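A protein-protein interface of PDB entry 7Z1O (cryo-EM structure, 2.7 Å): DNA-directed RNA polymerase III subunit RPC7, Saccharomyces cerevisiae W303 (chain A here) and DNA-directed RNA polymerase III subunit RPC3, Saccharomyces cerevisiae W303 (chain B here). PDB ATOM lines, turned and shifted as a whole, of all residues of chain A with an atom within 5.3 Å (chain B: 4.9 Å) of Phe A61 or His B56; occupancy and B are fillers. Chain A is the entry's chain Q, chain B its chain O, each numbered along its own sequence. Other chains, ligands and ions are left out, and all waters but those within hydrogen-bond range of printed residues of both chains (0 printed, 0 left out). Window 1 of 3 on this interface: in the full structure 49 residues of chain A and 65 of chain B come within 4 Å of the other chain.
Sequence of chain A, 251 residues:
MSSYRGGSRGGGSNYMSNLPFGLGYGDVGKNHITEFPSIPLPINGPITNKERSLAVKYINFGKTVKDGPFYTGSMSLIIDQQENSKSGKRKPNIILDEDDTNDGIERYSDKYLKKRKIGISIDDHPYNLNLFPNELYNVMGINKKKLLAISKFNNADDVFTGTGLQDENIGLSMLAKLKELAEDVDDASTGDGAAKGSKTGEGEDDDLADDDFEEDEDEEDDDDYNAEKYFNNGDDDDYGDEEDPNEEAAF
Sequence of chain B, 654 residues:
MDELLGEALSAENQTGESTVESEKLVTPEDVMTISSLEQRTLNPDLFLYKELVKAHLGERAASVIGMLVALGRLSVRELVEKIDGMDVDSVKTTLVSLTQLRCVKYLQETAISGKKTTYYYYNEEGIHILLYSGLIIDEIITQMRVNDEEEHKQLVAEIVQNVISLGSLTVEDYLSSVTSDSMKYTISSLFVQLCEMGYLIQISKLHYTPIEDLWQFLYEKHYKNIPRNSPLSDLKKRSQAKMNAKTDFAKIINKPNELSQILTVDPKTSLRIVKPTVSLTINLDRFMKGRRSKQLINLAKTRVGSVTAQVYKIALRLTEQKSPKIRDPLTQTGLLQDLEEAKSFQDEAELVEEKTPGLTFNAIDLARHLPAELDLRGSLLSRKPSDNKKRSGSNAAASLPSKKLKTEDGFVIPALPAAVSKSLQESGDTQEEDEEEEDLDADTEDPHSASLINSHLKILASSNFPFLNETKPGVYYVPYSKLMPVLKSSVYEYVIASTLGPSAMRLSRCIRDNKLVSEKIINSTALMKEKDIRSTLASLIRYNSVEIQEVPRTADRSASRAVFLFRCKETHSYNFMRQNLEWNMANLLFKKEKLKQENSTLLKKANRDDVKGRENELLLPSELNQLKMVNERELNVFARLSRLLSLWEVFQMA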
ATOM      1  N   VAL A  56      -2.248  -2.463 -33.762  1.00  0.00           N
ATOM      2  CA  VAL A  56      -0.925  -2.675 -34.342  1.00  0.00           C
ATOM      3  C   VAL A  56       0.136  -2.684 -33.244  1.00  0.00           C
ATOM      4  O   VAL A  56       1.171  -3.345 -33.383  1.00  0.00           O
ATOM      5  CB  VAL A  56      -0.622  -1.645 -35.453  1.00  0.00           C
ATOM      6  CG1 VAL A  56      -0.438  -0.250 -34.903  1.00  0.00           C
ATOM      7  CG2 VAL A  56       0.589  -2.071 -36.275  1.00  0.00           C
ATOM      8  N   LYS A  57      -0.117  -2.005 -32.118  1.00  0.00           N
ATOM      9  CA  LYS A  57       0.764  -2.148 -30.959  1.00  0.00           C
ATOM     10  C   LYS A  57       0.720  -3.570 -30.405  1.00  0.00           C
ATOM     11  O   LYS A  57       1.760  -4.146 -30.059  1.00  0.00           O
ATOM     12  CB  LYS A  57       0.383  -1.134 -29.881  1.00  0.00           C
ATOM     13  CG  LYS A  57       0.896   0.270 -30.144  1.00  0.00           C
ATOM     14  CD  LYS A  57       0.444   1.237 -29.067  1.00  0.00           C
ATOM     15  CE  LYS A  57       1.057   2.611 -29.268  1.00  0.00           C
ATOM     16  NZ  LYS A  57       0.689   3.194 -30.587  1.00  0.00           N
ATOM     17  N   TYR A  58      -0.484  -4.148 -30.308  1.00  0.00           N
ATOM     18  CA  TYR A  58      -0.623  -5.558 -29.939  1.00  0.00           C
ATOM     19  C   TYR A  58       0.164  -6.474 -30.871  1.00  0.00           C
ATOM     20  O   TYR A  58       0.887  -7.370 -30.417  1.00  0.00           O
ATOM     21  CB  TYR A  58      -2.099  -5.966 -29.938  1.00  0.00           C
ATOM     22  CG  TYR A  58      -2.881  -5.637 -28.686  1.00  0.00           C
ATOM     23  CD1 TYR A  58      -2.244  -5.396 -27.482  1.00  0.00           C
ATOM     24  CD2 TYR A  58      -4.266  -5.581 -28.710  1.00  0.00           C
ATOM     25  CE1 TYR A  58      -2.966  -5.117 -26.340  1.00  0.00           C
ATOM     26  CE2 TYR A  58      -4.992  -5.300 -27.575  1.00  0.00           C
ATOM     27  CZ  TYR A  58      -4.335  -5.062 -26.394  1.00  0.00           C
ATOM     28  OH  TYR A  58      -5.054  -4.774 -25.258  1.00  0.00           O
ATOM     29  N   ILE A  59       0.019  -6.268 -32.183  1.00  0.00           N
ATOM     30  CA  ILE A  59       0.693  -7.127 -33.158  1.00  0.00           C
ATOM     31  C   ILE A  59       2.206  -6.984 -33.045  1.00  0.00           C
ATOM     32  O   ILE A  59       2.944  -7.979 -33.086  1.00  0.00           O
ATOM     33  CB  ILE A  59       0.197  -6.814 -34.582  1.00  0.00           C
ATOM     34  CG1 ILE A  59      -1.291  -7.129 -34.706  1.00  0.00           C
ATOM     35  CG2 ILE A  59       0.989  -7.600 -35.614  1.00  0.00           C
ATOM     36  CD1 ILE A  59      -1.838  -6.961 -36.099  1.00  0.00           C
ATOM     37  N   ASN A  60       2.689  -5.748 -32.894  1.00  0.00           N
ATOM     38  CA  ASN A  60       4.122  -5.510 -32.766  1.00  0.00           C
ATOM     39  C   ASN A  60       4.684  -6.162 -31.511  1.00  0.00           C
ATOM     40  O   ASN A  60       5.767  -6.759 -31.547  1.00  0.00           O
ATOM     41  CB  ASN A  60       4.397  -4.008 -32.757  1.00  0.00           C
ATOM     42  CG  ASN A  60       4.512  -3.431 -34.149  1.00  0.00           C
ATOM     43  OD1 ASN A  60       4.182  -4.089 -35.136  1.00  0.00           O
ATOM     44  ND2 ASN A  60       4.971  -2.190 -34.237  1.00  0.00           N
ATOM     45  N   PHE A  61       3.966  -6.059 -30.387  1.00  0.00           N
ATOM     46  CA  PHE A  61       4.438  -6.692 -29.160  1.00  0.00           C
ATOM     47  C   PHE A  61       4.448  -8.210 -29.282  1.00  0.00           C
ATOM     48  O   PHE A  61       5.393  -8.869 -28.828  1.00  0.00           O
ATOM     49  CB  PHE A  61       3.583  -6.264 -27.974  1.00  0.00           C
ATOM     50  CG  PHE A  61       3.961  -6.942 -26.695  1.00  0.00           C
ATOM     51  CD1 PHE A  61       5.115  -6.581 -26.027  1.00  0.00           C
ATOM     52  CD2 PHE A  61       3.175  -7.952 -26.169  1.00  0.00           C
ATOM     53  CE1 PHE A  61       5.473  -7.206 -24.857  1.00  0.00           C
ATOM     54  CE2 PHE A  61       3.530  -8.580 -24.993  1.00  0.00           C
ATOM     55  CZ  PHE A  61       4.677  -8.205 -24.335  1.00  0.00           C
ATOM     56  N   GLY A  62       3.404  -8.783 -29.885  1.00  0.00           N
ATOM     57  CA  GLY A  62       3.381 -10.224 -30.083  1.00  0.00           C
ATOM     58  C   GLY A  62       4.519 -10.704 -30.961  1.00  0.00           C
ATOM     59  O   GLY A  62       5.141 -11.732 -30.682  1.00  0.00           O
ATOM     60  N   LYS A  63       4.824  -9.951 -32.020  1.00  0.00           N
ATOM     61  CA  LYS A  63       5.931 -10.320 -32.895  1.00  0.00           C
ATOM     62  C   LYS A  63       7.274 -10.175 -32.189  1.00  0.00           C
ATOM     63  O   LYS A  63       8.160 -11.021 -32.357  1.00  0.00           O
ATOM     64  CB  LYS A  63       5.897  -9.478 -34.169  1.00  0.00           C
ATOM     65  CG  LYS A  63       6.991  -9.819 -35.165  1.00  0.00           C
ATOM     66  CD  LYS A  63       6.819  -9.051 -36.464  1.00  0.00           C
ATOM     67  CE  LYS A  63       7.148  -7.581 -36.279  1.00  0.00           C
ATOM     68  NZ  LYS A  63       8.600  -7.372 -36.019  1.00  0.00           N
ATOM     69  N   THR A  64       7.447  -9.119 -31.386  1.00  0.00           N
ATOM     70  CA  THR A  64       8.744  -8.900 -30.751  1.00  0.00           C
ATOM     71  C   THR A  64       8.967  -9.842 -29.574  1.00  0.00           C
ATOM     72  O   THR A  64      10.113 -10.044 -29.158  1.00  0.00           O
ATOM     73  CB  THR A  64       8.896  -7.440 -30.312  1.00  0.00           C
ATOM     74  OG1 THR A  64      10.279  -7.159 -30.079  1.00  0.00           O
ATOM     75  CG2 THR A  64       8.124  -7.158 -29.037  1.00  0.00           C
ATOM     76  N   VAL A  65       7.899 -10.424 -29.022  1.00  0.00           N
ATOM     77  CA  VAL A  65       8.091 -11.484 -28.037  1.00  0.00           C
ATOM     78  C   VAL A  65       8.254 -12.829 -28.739  1.00  0.00           C
ATOM     79  O   VAL A  65       8.931 -13.730 -28.228  1.00  0.00           O
ATOM     80  CB  VAL A  65       6.926 -11.477 -27.026  1.00  0.00           C
ATOM     81  CG1 VAL A  65       7.028 -12.629 -26.040  1.00  0.00           C
ATOM     82  CG2 VAL A  65       6.916 -10.169 -26.269  1.00  0.00           C
ATOM     83  N   LYS A  66       7.677 -12.968 -29.938  1.00  0.00           N
ATOM     84  CA  LYS A  66       7.767 -14.223 -30.681  1.00  0.00           C
ATOM     85  C   LYS A  66       9.208 -14.560 -31.050  1.00  0.00           C
ATOM     86  O   LYS A  66       9.623 -15.721 -30.959  1.00  0.00           O
ATOM     87  CB  LYS A  66       6.902 -14.138 -31.938  1.00  0.00           C
ATOM     88  CG  LYS A  66       6.818 -15.424 -32.740  1.00  0.00           C
ATOM     89  CD  LYS A  66       5.852 -16.406 -32.106  1.00  0.00           C
ATOM     90  CE  LYS A  66       4.410 -15.996 -32.354  1.00  0.00           C
ATOM     91  NZ  LYS A  66       3.451 -16.999 -31.819  1.00  0.00           N
ATOM     92  N   TYR A  71      11.334 -17.621 -25.899  1.00  0.00           N
ATOM     93  CA  TYR A  71      10.220 -18.126 -26.691  1.00  0.00           C
ATOM     94  C   TYR A  71       9.797 -19.522 -26.267  1.00  0.00           C
ATOM     95  O   TYR A  71       8.618 -19.730 -25.953  1.00  0.00           O
ATOM     96  CB  TYR A  71      10.577 -18.111 -28.186  1.00  0.00           C
ATOM     97  CG  TYR A  71       9.482 -18.657 -29.073  1.00  0.00           C
ATOM     98  CD1 TYR A  71       8.176 -18.206 -28.949  1.00  0.00           C
ATOM     99  CD2 TYR A  71       9.755 -19.614 -30.040  1.00  0.00           C
ATOM    100  CE1 TYR A  71       7.171 -18.699 -29.752  1.00  0.00           C
ATOM    101  CE2 TYR A  71       8.755 -20.110 -30.853  1.00  0.00           C
ATOM    102  CZ  TYR A  71       7.465 -19.649 -30.704  1.00  0.00           C
ATOM    103  OH  TYR A  71       6.465 -20.141 -31.510  1.00  0.00           O
ATOM    104  N   LEU B  52      -2.976 -17.050 -23.873  1.00  0.00           N
ATOM    105  CA  LEU B  52      -2.060 -15.912 -23.899  1.00  0.00           C
ATOM    106  C   LEU B  52      -0.605 -16.369 -23.925  1.00  0.00           C
ATOM    107  O   LEU B  52       0.210 -15.850 -24.701  1.00  0.00           O
ATOM    108  CB  LEU B  52      -2.317 -15.005 -22.698  1.00  0.00           C
ATOM    109  CG  LEU B  52      -3.436 -13.980 -22.853  1.00  0.00           C
ATOM    110  CD1 LEU B  52      -3.962 -13.561 -21.496  1.00  0.00           C
ATOM    111  CD2 LEU B  52      -2.946 -12.775 -23.634  1.00  0.00           C
ATOM    112  N   VAL B  53      -0.265 -17.355 -23.091  1.00  0.00           N
ATOM    113  CA  VAL B  53       1.114 -17.828 -23.036  1.00  0.00           C
ATOM    114  C   VAL B  53       1.490 -18.541 -24.331  1.00  0.00           C
ATOM    115  O   VAL B  53       2.612 -18.393 -24.830  1.00  0.00           O
ATOM    116  CB  VAL B  53       1.320 -18.718 -21.797  1.00  0.00           C
ATOM    117  CG1 VAL B  53       2.682 -19.372 -21.821  1.00  0.00           C
ATOM    118  CG2 VAL B  53       1.176 -17.890 -20.538  1.00  0.00           C
ATOM    119  N   LYS B  54       0.559 -19.298 -24.918  1.00  0.00           N
ATOM    120  CA  LYS B  54       0.846 -19.971 -26.180  1.00  0.00           C
ATOM    121  C   LYS B  54       0.951 -18.978 -27.331  1.00  0.00           C
ATOM    122  O   LYS B  54       1.665 -19.227 -28.308  1.00  0.00           O
ATOM    123  CB  LYS B  54      -0.230 -21.015 -26.473  1.00  0.00           C
ATOM    124  CG  LYS B  54       0.219 -22.124 -27.404  1.00  0.00           C
ATOM    125  CD  LYS B  54      -0.942 -23.020 -27.788  1.00  0.00           C
ATOM    126  CE  LYS B  54      -1.513 -23.732 -26.575  1.00  0.00           C
ATOM    127  NZ  LYS B  54      -2.856 -24.309 -26.853  1.00  0.00           N
ATOM    128  N   ALA B  55       0.231 -17.858 -27.246  1.00  0.00           N
ATOM    129  CA  ALA B  55       0.317 -16.853 -28.297  1.00  0.00           C
ATOM    130  C   ALA B  55       1.632 -16.088 -28.227  1.00  0.00           C
ATOM    131  O   ALA B  55       2.263 -15.837 -29.259  1.00  0.00           O
ATOM    132  CB  ALA B  55      -0.866 -15.892 -28.202  1.00  0.00           C
ATOM    133  N   HIS B  56       2.064 -15.712 -27.024  1.00  0.00           N
ATOM    134  CA  HIS B  56       3.274 -14.905 -26.896  1.00  0.00           C
ATOM    135  C   HIS B  56       4.525 -15.773 -26.775  1.00  0.00           C
ATOM    136  O   HIS B  56       5.452 -15.650 -27.583  1.00  0.00           O
ATOM    137  CB  HIS B  56       3.138 -13.952 -25.706  1.00  0.00           C
ATOM    138  CG  HIS B  56       2.141 -12.860 -25.932  1.00  0.00           C
ATOM    139  ND1 HIS B  56       0.789 -13.098 -26.039  1.00  0.00           N
ATOM    140  CD2 HIS B  56       2.301 -11.526 -26.090  1.00  0.00           C
ATOM    141  CE1 HIS B  56       0.157 -11.957 -26.243  1.00  0.00           C
ATOM    142  NE2 HIS B  56       1.052 -10.986 -26.278  1.00  0.00           N
ATOM    143  N   LEU B  57       4.568 -16.648 -25.777  1.00  0.00           N
ATOM    144  CA  LEU B  57       5.631 -17.632 -25.671  1.00  0.00           C
ATOM    145  C   LEU B  57       5.223 -18.891 -26.434  1.00  0.00           C
ATOM    146  O   LEU B  57       4.258 -18.895 -27.200  1.00  0.00           O
ATOM    147  CB  LEU B  57       5.944 -17.925 -24.206  1.00  0.00           C
ATOM    148  CG  LEU B  57       6.102 -16.697 -23.304  1.00  0.00           C
ATOM    149  CD1 LEU B  57       6.451 -17.108 -21.891  1.00  0.00           C
ATOM    150  CD2 LEU B  57       7.150 -15.747 -23.849  1.00  0.00           C
ATOM    151  N   GLY B  58       5.963 -19.976 -26.234  1.00  0.00           N
ATOM    152  CA  GLY B  58       5.730 -21.193 -26.979  1.00  0.00           C
ATOM    153  C   GLY B  58       4.760 -22.141 -26.298  1.00  0.00           C
ATOM    154  O   GLY B  58       4.114 -21.824 -25.298  1.00  0.00           O
ATOM    155  N   LEU B 130       0.969  -9.379 -20.250  1.00  0.00           N
ATOM    156  CA  LEU B 130       0.888  -9.850 -21.631  1.00  0.00           C
ATOM    157  C   LEU B 130      -0.439  -9.460 -22.272  1.00  0.00           C
ATOM    158  O   LEU B 130      -0.487  -9.108 -23.456  1.00  0.00           O
ATOM    159  CB  LEU B 130       1.075 -11.366 -21.683  1.00  0.00           C
ATOM    160  CG  LEU B 130       2.465 -11.911 -21.362  1.00  0.00           C
ATOM    161  CD1 LEU B 130       2.488 -13.419 -21.521  1.00  0.00           C
ATOM    162  CD2 LEU B 130       3.512 -11.261 -22.250  1.00  0.00           C
ATOM    163  N   SER B 133      -0.737  -5.365 -22.865  1.00  0.00           N
ATOM    164  CA  SER B 133       0.551  -4.800 -23.269  1.00  0.00           C
ATOM    165  C   SER B 133       0.390  -3.558 -24.141  1.00  0.00           C
ATOM    166  O   SER B 133       0.976  -2.506 -23.860  1.00  0.00           O
ATOM    167  CB  SER B 133       1.371  -5.862 -23.996  1.00  0.00           C
ATOM    168  OG  SER B 133       2.665  -5.373 -24.303  1.00  0.00           O
ATOM    169  N   GLN B 161       8.125  -0.894 -24.560  1.00  0.00           N
ATOM    170  CA  GLN B 161       7.991  -2.173 -25.246  1.00  0.00           C
ATOM    171  C   GLN B 161       9.120  -3.123 -24.867  1.00  0.00           C
ATOM    172  O   GLN B 161       8.884  -4.314 -24.640  1.00  0.00           O
ATOM    173  CB  GLN B 161       7.955  -1.950 -26.756  1.00  0.00           C
ATOM    174  CG  GLN B 161       7.869  -3.220 -27.579  1.00  0.00           C
ATOM    175  CD  GLN B 161       7.461  -2.950 -29.011  1.00  0.00           C
ATOM    176  OE1 GLN B 161       6.290  -2.701 -29.298  1.00  0.00           O
ATOM    177  NE2 GLN B 161       8.426  -2.996 -29.920  1.00  0.00           N
ATOM    178  N   ILE B 164       8.517  -4.376 -21.216  1.00  0.00           N
ATOM    179  CA  ILE B 164       7.464  -5.385 -21.131  1.00  0.00           C
ATOM    180  C   ILE B 164       7.909  -6.692 -21.782  1.00  0.00           C
ATOM    181  O   ILE B 164       7.625  -7.782 -21.268  1.00  0.00           O
ATOM    182  CB  ILE B 164       6.159  -4.854 -21.752  1.00  0.00           C
ATOM    183  CG1 ILE B 164       5.690  -3.601 -21.023  1.00  0.00           C
ATOM    184  CG2 ILE B 164       5.060  -5.881 -21.652  1.00  0.00           C
ATOM    185  CD1 ILE B 164       4.517  -2.938 -21.690  1.00  0.00           C
ATOM    186  N   SER B 165       8.620  -6.613 -22.911  1.00  0.00           N
ATOM    187  CA  SER B 165       9.011  -7.822 -23.627  1.00  0.00           C
ATOM    188  C   SER B 165      10.080  -8.604 -22.874  1.00  0.00           C
ATOM    189  O   SER B 165      10.032  -9.839 -22.826  1.00  0.00           O
ATOM    190  CB  SER B 165       9.501  -7.464 -25.029  1.00  0.00           C
ATOM    191  OG  SER B 165      10.710  -6.728 -24.972  1.00  0.00           O
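Of the printed residues of chain B, Phe A61 touches His B56, Leu B130, Ser B133, Ile B164 and Ser B165. Of chain A, only Phe A61 (3.4 Å), Val A65 (3.7 Å) and Tyr A71 (3.98 Å) come within 4 Å of His B56. Of the printed residues of chain A, Gly B58 touches Tyr A71. Printed residues of chain A within 4 Å of Leu B57: Val A65 and Tyr A71. Printed residues of chain B within 4 Å of Tyr A71: His B56 (3.98 Å), Leu B57 (3.5 Å) and Gly B58 (2.7 Å). Of the printed residues of chain A, Ser B133 touches Phe A61 (3.1 Å). Of the printed residues of chain A, Ile B164 touches Phe A61 (3.5 Å). Leu B52 touches none of the printed residues of chain A. Val B53 touches none of the printed residues of chain A. The nearest residue of chain B that does not touch Phe A61 is Gln B161 (4.2 Å). The nearest residue of chain A that does not touch His B56 is Lys A66 (4.1 Å).
Among the printed residues, merely in contact across the chains: Phe A61 with Ser B133, Phe A61 with His B56, Phe A61 with Ile B164, Tyr A71 with Leu B57, Val A65 with His B56, Phe A61 with Ser B165, Val A65 with Leu B57, Phe A61 with Leu B130, Val A65 with Ser B165 and Tyr A71 with His B56.
Of the 12 printed residues of chain B, 8 touch a printed residue of chain A. Printed residues of chain B that touch a printed residue of chain A: Ala B55, His B56, Leu B57, Gly B58, Leu B130, Ser B133, Ile B164 and Ser B165. Hydrophobic or aromatic side chains of chain B within 4 Å of the printed part of chain A: His B56, Leu B57, Leu B130 and Ile B164. Hydrophobic or aromatic side chains of chain A that line the printed part of chain B: Phe A61, Val A65 and Tyr A71. Among the printed residues, no Asp or Glu carboxylate lies within 4 Å of a Lys or Arg side-chain nitrogen of the other chain.
The side-chain amino group (NZ) of Lys A66 is in hydrogen-bond range of the backbone carbonyl oxygen (O) of Ala B55 (3.1 Å). N of Gly B58 lies within hydrogen-bond range of O of Tyr A71 (2.7 Å).
O of Gln B161 sits at hydrogen-bond distance from OG of Ser B165 (3.0 Å). ND1 of His B56 lies within hydrogen-bond range of O of Leu B52.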
